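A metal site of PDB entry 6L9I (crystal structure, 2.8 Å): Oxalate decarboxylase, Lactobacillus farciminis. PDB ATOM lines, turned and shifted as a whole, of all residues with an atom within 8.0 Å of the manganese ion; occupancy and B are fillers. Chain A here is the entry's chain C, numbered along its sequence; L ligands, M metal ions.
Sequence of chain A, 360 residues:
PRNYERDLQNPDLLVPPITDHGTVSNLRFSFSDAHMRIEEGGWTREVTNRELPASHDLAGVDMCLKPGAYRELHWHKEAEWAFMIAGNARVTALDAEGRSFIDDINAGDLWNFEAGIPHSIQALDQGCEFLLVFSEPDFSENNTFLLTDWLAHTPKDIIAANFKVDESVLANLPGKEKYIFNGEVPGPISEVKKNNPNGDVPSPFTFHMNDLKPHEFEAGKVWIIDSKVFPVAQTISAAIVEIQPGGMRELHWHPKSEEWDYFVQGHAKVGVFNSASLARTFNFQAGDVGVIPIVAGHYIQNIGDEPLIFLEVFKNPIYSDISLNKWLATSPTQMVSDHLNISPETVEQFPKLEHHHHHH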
ATOM      1  N   MET A  63     -29.219   6.209 -12.276  1.00  0.00           N
ATOM      2  CA  MET A  63     -29.244   5.119 -11.311  1.00  0.00           C
ATOM      3  C   MET A  63     -30.514   5.168 -10.474  1.00  0.00           C
ATOM      4  O   MET A  63     -31.007   6.258 -10.147  1.00  0.00           O
ATOM      5  CB  MET A  63     -28.010   5.181 -10.406  1.00  0.00           C
ATOM      6  CG  MET A  63     -27.899   4.029  -9.440  1.00  0.00           C
ATOM      7  SD  MET A  63     -26.346   4.061  -8.528  1.00  0.00           S
ATOM      8  CE  MET A  63     -25.264   3.250  -9.704  1.00  0.00           C
ATOM      9  N   ARG A  71     -26.145   1.665  -2.632  1.00  0.00           N
ATOM     10  CA  ARG A  71     -25.105   1.820  -3.634  1.00  0.00           C
ATOM     11  C   ARG A  71     -23.796   1.577  -2.902  1.00  0.00           C
ATOM     12  O   ARG A  71     -23.414   2.362  -2.027  1.00  0.00           O
ATOM     13  CB  ARG A  71     -25.169   3.215  -4.265  1.00  0.00           C
ATOM     14  CG  ARG A  71     -24.074   3.504  -5.258  1.00  0.00           C
ATOM     15  CD  ARG A  71     -23.870   2.342  -6.216  1.00  0.00           C
ATOM     16  NE  ARG A  71     -22.800   2.608  -7.170  1.00  0.00           N
ATOM     17  CZ  ARG A  71     -21.742   1.830  -7.316  1.00  0.00           C
ATOM     18  NH1 ARG A  71     -21.616   0.733  -6.585  1.00  0.00           N
ATOM     19  NH2 ARG A  71     -20.806   2.141  -8.202  1.00  0.00           N
ATOM     20  N   GLU A  72     -23.106   0.479  -3.240  1.00  0.00           N
ATOM     21  CA  GLU A  72     -22.024  -0.005  -2.396  1.00  0.00           C
ATOM     22  C   GLU A  72     -20.940   1.044  -2.197  1.00  0.00           C
ATOM     23  O   GLU A  72     -20.649   1.847  -3.099  1.00  0.00           O
ATOM     24  CB  GLU A  72     -21.413  -1.282  -2.986  1.00  0.00           C
ATOM     25  CG  GLU A  72     -20.238  -1.818  -2.181  1.00  0.00           C
ATOM     26  CD  GLU A  72     -19.540  -2.975  -2.855  1.00  0.00           C
ATOM     27  OE1 GLU A  72     -20.129  -3.582  -3.771  1.00  0.00           O
ATOM     28  OE2 GLU A  72     -18.395  -3.269  -2.463  1.00  0.00           O
ATOM     29  N   LEU A  73     -20.356   1.047  -1.006  1.00  0.00           N
ATOM     30  CA  LEU A  73     -19.202   1.873  -0.668  1.00  0.00           C
ATOM     31  C   LEU A  73     -18.124   1.789  -1.744  1.00  0.00           C
ATOM     32  O   LEU A  73     -17.683   0.695  -2.099  1.00  0.00           O
ATOM     33  CB  LEU A  73     -18.628   1.409   0.678  1.00  0.00           C
ATOM     34  CG  LEU A  73     -19.499   1.745   1.880  1.00  0.00           C
ATOM     35  CD1 LEU A  73     -19.016   1.040   3.135  1.00  0.00           C
ATOM     36  CD2 LEU A  73     -19.400   3.219   2.048  1.00  0.00           C
ATOM     37  N   HIS A  74     -17.691   2.945  -2.232  1.00  0.00           N
ATOM     38  CA  HIS A  74     -16.794   2.969  -3.375  1.00  0.00           C
ATOM     39  C   HIS A  74     -16.116   4.331  -3.488  1.00  0.00           C
ATOM     40  O   HIS A  74     -16.423   5.278  -2.753  1.00  0.00           O
ATOM     41  CB  HIS A  74     -17.539   2.638  -4.676  1.00  0.00           C
ATOM     42  CG  HIS A  74     -18.528   3.684  -5.072  1.00  0.00           C
ATOM     43  ND1 HIS A  74     -19.858   3.634  -4.687  1.00  0.00           N
ATOM     44  CD2 HIS A  74     -18.399   4.808  -5.816  1.00  0.00           C
ATOM     45  CE1 HIS A  74     -20.494   4.689  -5.178  1.00  0.00           C
ATOM     46  NE2 HIS A  74     -19.627   5.411  -5.865  1.00  0.00           N
ATOM     47  N   TRP A  75     -15.186   4.415  -4.452  1.00  0.00           N
ATOM     48  CA  TRP A  75     -14.535   5.660  -4.840  1.00  0.00           C
ATOM     49  C   TRP A  75     -14.104   5.519  -6.294  1.00  0.00           C
ATOM     50  O   TRP A  75     -14.116   4.427  -6.860  1.00  0.00           O
ATOM     51  CB  TRP A  75     -13.360   6.001  -3.914  1.00  0.00           C
ATOM     52  CG  TRP A  75     -12.103   5.149  -4.044  1.00  0.00           C
ATOM     53  CD1 TRP A  75     -10.929   5.501  -4.646  1.00  0.00           C
ATOM     54  CD2 TRP A  75     -11.881   3.820  -3.506  1.00  0.00           C
ATOM     55  NE1 TRP A  75     -10.012   4.495  -4.550  1.00  0.00           N
ATOM     56  CE2 TRP A  75     -10.559   3.453  -3.847  1.00  0.00           C
ATOM     57  CE3 TRP A  75     -12.672   2.929  -2.784  1.00  0.00           C
ATOM     58  CZ2 TRP A  75     -10.027   2.218  -3.490  1.00  0.00           C
ATOM     59  CZ3 TRP A  75     -12.130   1.704  -2.424  1.00  0.00           C
ATOM     60  CH2 TRP A  75     -10.818   1.360  -2.782  1.00  0.00           C
ATOM     61  N   HIS A  76     -13.692   6.639  -6.891  1.00  0.00           N
ATOM     62  CA  HIS A  76     -13.196   6.606  -8.256  1.00  0.00           C
ATOM     63  C   HIS A  76     -12.271   7.781  -8.514  1.00  0.00           C
ATOM     64  O   HIS A  76     -12.255   8.765  -7.777  1.00  0.00           O
ATOM     65  CB  HIS A  76     -14.352   6.602  -9.274  1.00  0.00           C
ATOM     66  CG  HIS A  76     -15.492   7.481  -8.903  1.00  0.00           C
ATOM     67  ND1 HIS A  76     -16.506   7.067  -8.061  1.00  0.00           N
ATOM     68  CD2 HIS A  76     -15.802   8.752  -9.269  1.00  0.00           C
ATOM     69  CE1 HIS A  76     -17.379   8.053  -7.924  1.00  0.00           C
ATOM     70  NE2 HIS A  76     -16.975   9.077  -8.639  1.00  0.00           N
ATOM     71  N   GLU A  78     -12.467   9.902 -10.855  1.00  0.00           N
ATOM     72  CA  GLU A  78     -13.223  11.052 -11.347  1.00  0.00           C
ATOM     73  C   GLU A  78     -14.036  11.676 -10.230  1.00  0.00           C
ATOM     74  O   GLU A  78     -14.215  11.097  -9.154  1.00  0.00           O
ATOM     75  CB  GLU A  78     -14.133  10.631 -12.501  1.00  0.00           C
ATOM     76  CG  GLU A  78     -13.359  10.024 -13.663  1.00  0.00           C
ATOM     77  CD  GLU A  78     -13.380   8.513 -13.675  1.00  0.00           C
ATOM     78  OE1 GLU A  78     -13.689   7.907 -12.629  1.00  0.00           O
ATOM     79  OE2 GLU A  78     -13.066   7.930 -14.737  1.00  0.00           O
ATOM     80  N   ALA A  79     -14.490  12.901 -10.469  1.00  0.00           N
ATOM     81  CA  ALA A  79     -15.381  13.592  -9.559  1.00  0.00           C
ATOM     82  C   ALA A  79     -16.834  13.269  -9.891  1.00  0.00           C
ATOM     83  O   ALA A  79     -17.206  13.098 -11.059  1.00  0.00           O
ATOM     84  CB  ALA A  79     -15.153  15.104  -9.606  1.00  0.00           C
ATOM     85  N   GLU A  80     -17.664  13.213  -8.852  1.00  0.00           N
ATOM     86  CA  GLU A  80     -19.080  12.903  -8.935  1.00  0.00           C
ATOM     87  C   GLU A  80     -19.891  14.160  -8.662  1.00  0.00           C
ATOM     88  O   GLU A  80     -19.699  14.829  -7.639  1.00  0.00           O
ATOM     89  CB  GLU A  80     -19.475  11.832  -7.926  1.00  0.00           C
ATOM     90  CG  GLU A  80     -20.427  10.780  -8.439  1.00  0.00           C
ATOM     91  CD  GLU A  80     -20.982   9.883  -7.335  1.00  0.00           C
ATOM     92  OE1 GLU A  80     -21.911  10.334  -6.628  1.00  0.00           O
ATOM     93  OE2 GLU A  80     -20.498   8.745  -7.178  1.00  0.00           O
ATOM     94  N   TRP A 111     -25.568  16.389  -4.803  1.00  0.00           N
ATOM     95  CA  TRP A 111     -24.395  16.094  -3.997  1.00  0.00           C
ATOM     96  C   TRP A 111     -23.162  16.141  -4.889  1.00  0.00           C
ATOM     97  O   TRP A 111     -23.256  16.190  -6.119  1.00  0.00           O
ATOM     98  CB  TRP A 111     -24.536  14.747  -3.264  1.00  0.00           C
ATOM     99  CG  TRP A 111     -24.400  13.484  -4.084  1.00  0.00           C
ATOM    100  CD1 TRP A 111     -23.263  12.995  -4.657  1.00  0.00           C
ATOM    101  CD2 TRP A 111     -25.422  12.506  -4.341  1.00  0.00           C
ATOM    102  NE1 TRP A 111     -23.524  11.798  -5.282  1.00  0.00           N
ATOM    103  CE2 TRP A 111     -24.843  11.468  -5.090  1.00  0.00           C
ATOM    104  CE3 TRP A 111     -26.773  12.420  -4.015  1.00  0.00           C
ATOM    105  CZ2 TRP A 111     -25.573  10.368  -5.537  1.00  0.00           C
ATOM    106  CZ3 TRP A 111     -27.498  11.322  -4.455  1.00  0.00           C
ATOM    107  CH2 TRP A 111     -26.903  10.318  -5.203  1.00  0.00           C
ATOM    108  N   PHE A 113     -18.870  14.814  -4.861  1.00  0.00           N
ATOM    109  CA  PHE A 113     -17.664  14.219  -4.305  1.00  0.00           C
ATOM    110  C   PHE A 113     -16.512  14.459  -5.277  1.00  0.00           C
ATOM    111  O   PHE A 113     -16.518  13.916  -6.387  1.00  0.00           O
ATOM    112  CB  PHE A 113     -17.837  12.723  -4.060  1.00  0.00           C
ATOM    113  CG  PHE A 113     -19.043  12.380  -3.249  1.00  0.00           C
ATOM    114  CD1 PHE A 113     -19.190  12.888  -1.973  1.00  0.00           C
ATOM    115  CD2 PHE A 113     -20.021  11.537  -3.746  1.00  0.00           C
ATOM    116  CE1 PHE A 113     -20.298  12.559  -1.208  1.00  0.00           C
ATOM    117  CE2 PHE A 113     -21.135  11.205  -2.988  1.00  0.00           C
ATOM    118  CZ  PHE A 113     -21.267  11.730  -1.716  1.00  0.00           C
ATOM    119  N   ILE A 117     -12.735  10.833  -3.370  1.00  0.00           N
ATOM    120  CA  ILE A 117     -13.415  10.928  -2.076  1.00  0.00           C
ATOM    121  C   ILE A 117     -14.366   9.747  -1.949  1.00  0.00           C
ATOM    122  O   ILE A 117     -15.289   9.609  -2.771  1.00  0.00           O
ATOM    123  CB  ILE A 117     -14.155  12.273  -1.937  1.00  0.00           C
ATOM    124  CG1 ILE A 117     -13.166  13.445  -1.994  1.00  0.00           C
ATOM    125  CG2 ILE A 117     -14.959  12.310  -0.651  1.00  0.00           C
ATOM    126  CD1 ILE A 117     -12.136  13.460  -0.873  1.00  0.00           C
ATOM    127  N   PRO A 118     -14.184   8.879  -0.961  1.00  0.00           N
ATOM    128  CA  PRO A 118     -15.054   7.699  -0.838  1.00  0.00           C
ATOM    129  C   PRO A 118     -16.426   8.075  -0.303  1.00  0.00           C
ATOM    130  O   PRO A 118     -16.581   9.034   0.443  1.00  0.00           O
ATOM    131  CB  PRO A 118     -14.291   6.818   0.156  1.00  0.00           C
ATOM    132  CG  PRO A 118     -13.522   7.784   0.992  1.00  0.00           C
ATOM    133  CD  PRO A 118     -13.179   8.958   0.112  1.00  0.00           C
ATOM    134  N   HIS A 119     -17.430   7.297  -0.709  1.00  0.00           N
ATOM    135  CA  HIS A 119     -18.806   7.667  -0.372  1.00  0.00           C
ATOM    136  C   HIS A 119     -19.735   6.467  -0.507  1.00  0.00           C
ATOM    137  O   HIS A 119     -19.385   5.422  -1.063  1.00  0.00           O
ATOM    138  CB  HIS A 119     -19.288   8.811  -1.257  1.00  0.00           C
ATOM    139  CG  HIS A 119     -19.131   8.571  -2.730  1.00  0.00           C
ATOM    140  ND1 HIS A 119     -17.987   8.899  -3.417  1.00  0.00           N
ATOM    141  CD2 HIS A 119     -19.970   8.034  -3.639  1.00  0.00           C
ATOM    142  CE1 HIS A 119     -18.132   8.571  -4.693  1.00  0.00           C
ATOM    143  NE2 HIS A 119     -19.332   8.051  -4.852  1.00  0.00           N
ATOM    144  N   SER A 120     -20.936   6.645   0.052  1.00  0.00           N
ATOM    145  CA  SER A 120     -22.035   5.695  -0.027  1.00  0.00           C
ATOM    146  C   SER A 120     -23.352   6.418  -0.299  1.00  0.00           C
ATOM    147  O   SER A 120     -23.552   7.567   0.102  1.00  0.00           O
ATOM    148  CB  SER A 120     -22.195   4.906   1.266  1.00  0.00           C
ATOM    149  OG  SER A 120     -22.909   5.712   2.190  1.00  0.00           O
ATOM    150  N   ILE A 121     -24.277   5.662  -0.893  1.00  0.00           N
ATOM    151  CA  ILE A 121     -25.657   6.090  -1.124  1.00  0.00           C
ATOM    152  C   ILE A 121     -26.589   4.951  -0.711  1.00  0.00           C
ATOM    153  O   ILE A 121     -26.340   3.788  -1.037  1.00  0.00           O
ATOM    154  CB  ILE A 121     -25.913   6.445  -2.607  1.00  0.00           C
ATOM    155  CG1 ILE A 121     -24.759   7.257  -3.190  1.00  0.00           C
ATOM    156  CG2 ILE A 121     -27.224   7.193  -2.741  1.00  0.00           C
ATOM    157  CD1 ILE A 121     -24.636   7.126  -4.700  1.00  0.00           C
ATOM    158  N   LEU A 132     -25.946  11.110 -12.086  1.00  0.00           N
ATOM    159  CA  LEU A 132     -24.575  11.371 -11.700  1.00  0.00           C
ATOM    160  C   LEU A 132     -23.809  11.851 -12.916  1.00  0.00           C
ATOM    161  O   LEU A 132     -23.997  11.332 -14.018  1.00  0.00           O
ATOM    162  CB  LEU A 132     -23.909  10.114 -11.129  1.00  0.00           C
ATOM    163  CG  LEU A 132     -24.730   9.278 -10.144  1.00  0.00           C
ATOM    164  CD1 LEU A 132     -23.913   8.116  -9.637  1.00  0.00           C
ATOM    165  CD2 LEU A 132     -25.164  10.146  -9.000  1.00  0.00           C
ATOM    166  N   PHE A 134     -19.821  12.607 -14.228  1.00  0.00           N
ATOM    167  CA  PHE A 134     -18.449  12.242 -13.930  1.00  0.00           C
ATOM    168  C   PHE A 134     -17.530  13.033 -14.858  1.00  0.00           C
ATOM    169  O   PHE A 134     -17.832  13.233 -16.041  1.00  0.00           O
ATOM    170  CB  PHE A 134     -18.218  10.739 -14.098  1.00  0.00           C
ATOM    171  CG  PHE A 134     -18.950   9.904 -13.096  1.00  0.00           C
ATOM    172  CD1 PHE A 134     -20.243   9.460 -13.341  1.00  0.00           C
ATOM    173  CD2 PHE A 134     -18.333   9.521 -11.914  1.00  0.00           C
ATOM    174  CE1 PHE A 134     -20.912   8.659 -12.420  1.00  0.00           C
ATOM    175  CE2 PHE A 134     -18.990   8.720 -11.001  1.00  0.00           C
ATOM    176  CZ  PHE A 134     -20.285   8.289 -11.250  1.00  0.00           C
ATOM    177  N   PHE A 139     -15.927   7.505 -18.534  1.00  0.00           N
ATOM    178  CA  PHE A 139     -16.245   6.854 -17.272  1.00  0.00           C
ATOM    179  C   PHE A 139     -17.090   5.592 -17.499  1.00  0.00           C
ATOM    180  O   PHE A 139     -17.735   5.427 -18.529  1.00  0.00           O
ATOM    181  CB  PHE A 139     -16.980   7.816 -16.339  1.00  0.00           C
ATOM    182  CG  PHE A 139     -17.403   7.188 -15.030  1.00  0.00           C
ATOM    183  CD1 PHE A 139     -16.537   7.141 -13.952  1.00  0.00           C
ATOM    184  CD2 PHE A 139     -18.677   6.646 -14.878  1.00  0.00           C
ATOM    185  CE1 PHE A 139     -16.925   6.569 -12.755  1.00  0.00           C
ATOM    186  CE2 PHE A 139     -19.063   6.064 -13.690  1.00  0.00           C
ATOM    187  CZ  PHE A 139     -18.188   6.031 -12.624  1.00  0.00           C
ATOM    188  N   GLU A 141     -19.470   2.916 -14.743  1.00  0.00           N
ATOM    189  CA  GLU A 141     -19.885   2.474 -13.418  1.00  0.00           C
ATOM    190  C   GLU A 141     -19.358   1.095 -13.059  1.00  0.00           C
ATOM    191  O   GLU A 141     -19.205   0.790 -11.873  1.00  0.00           O
ATOM    192  CB  GLU A 141     -21.419   2.475 -13.302  1.00  0.00           C
ATOM    193  CG  GLU A 141     -21.998   3.740 -12.702  1.00  0.00           C
ATOM    194  CD  GLU A 141     -21.656   3.880 -11.234  1.00  0.00           C
ATOM    195  OE1 GLU A 141     -21.516   5.040 -10.780  1.00  0.00           O
ATOM    196  OE2 GLU A 141     -21.533   2.853 -10.544  1.00  0.00           O
ATOM    197  N   THR A 144     -15.683   1.135 -10.977  1.00  0.00           N
ATOM    198  CA  THR A 144     -15.475   1.920  -9.773  1.00  0.00           C
ATOM    199  C   THR A 144     -14.825   1.045  -8.706  1.00  0.00           C
ATOM    200  O   THR A 144     -15.007  -0.178  -8.699  1.00  0.00           O
ATOM    201  CB  THR A 144     -16.789   2.530  -9.249  1.00  0.00           C
ATOM    202  OG1 THR A 144     -17.531   1.543  -8.531  1.00  0.00           O
ATOM    203  CG2 THR A 144     -17.611   3.074 -10.403  1.00  0.00           C
ATOM    204  N   PHE A 145     -14.124   1.680  -7.774  1.00  0.00           N
ATOM    205  CA  PHE A 145     -13.360   0.962  -6.762  1.00  0.00           C
ATOM    206  C   PHE A 145     -14.291   0.595  -5.613  1.00  0.00           C
ATOM    207  O   PHE A 145     -14.641   1.438  -4.792  1.00  0.00           O
ATOM    208  CB  PHE A 145     -12.200   1.811  -6.272  1.00  0.00           C
ATOM    209  CG  PHE A 145     -11.062   1.947  -7.254  1.00  0.00           C
ATOM    210  CD1 PHE A 145     -11.179   2.759  -8.376  1.00  0.00           C
ATOM    211  CD2 PHE A 145      -9.863   1.280  -7.044  1.00  0.00           C
ATOM    212  CE1 PHE A 145     -10.130   2.894  -9.274  1.00  0.00           C
ATOM    213  CE2 PHE A 145      -8.801   1.412  -7.936  1.00  0.00           C
ATOM    214  CZ  PHE A 145      -8.940   2.214  -9.052  1.00  0.00           C
HETATM  215  C1  LIG L   1     -22.023   5.742  -7.866  1.00  0.00           C
HETATM  216  O1  LIG L   1     -20.833   5.727  -8.195  1.00  0.00           O
HETATM  217  O2  LIG L   1     -22.898   5.114  -8.446  1.00  0.00           O
HETATM  218 MN    MN M   1     -19.516   7.022  -6.780  1.00  0.00          MN
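His 76 touches the manganese ion (CE1 to MN, 2.6 Å). Within 4 Å of the manganese ion: His 74, His 76, Glu 80 and His 119. The nearest printed residue that does not touch the manganese ion is Phe 134 (4.6 Å).
A ring nitrogen (NE2) of His 74 binds the manganese ion, 1.9 Å away. The manganese ion is bound by OE2 of Glu 80, 2.0 Å away. The manganese ion is bound by NE2 of His 119 (2.2 Å). O1 of the ligand binds the manganese ion (2.3 Å). The manganese ion has four donor atoms within binding distance.
A ring nitrogen (ND1) of His 74 is in hydrogen-bond range of the backbone carbonyl oxygen (O) of Glu 72 (2.5 Å). The backbone NH (N) of Glu 80 lies within hydrogen-bond range of the backbone carbonyl oxygen (O) of Phe 113 (2.8 Å). The side-chain carboxylate (OE1) of Glu 80 lies within hydrogen-bond range of the indole nitrogen (NE1) of Trp 111 (2.6 Å). O of Ile 117 is in hydrogen-bond range of ND1 of His 119, at 2.9 Å. O of Glu 78 sits close to NE2 of His 76 (3.5 Å).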
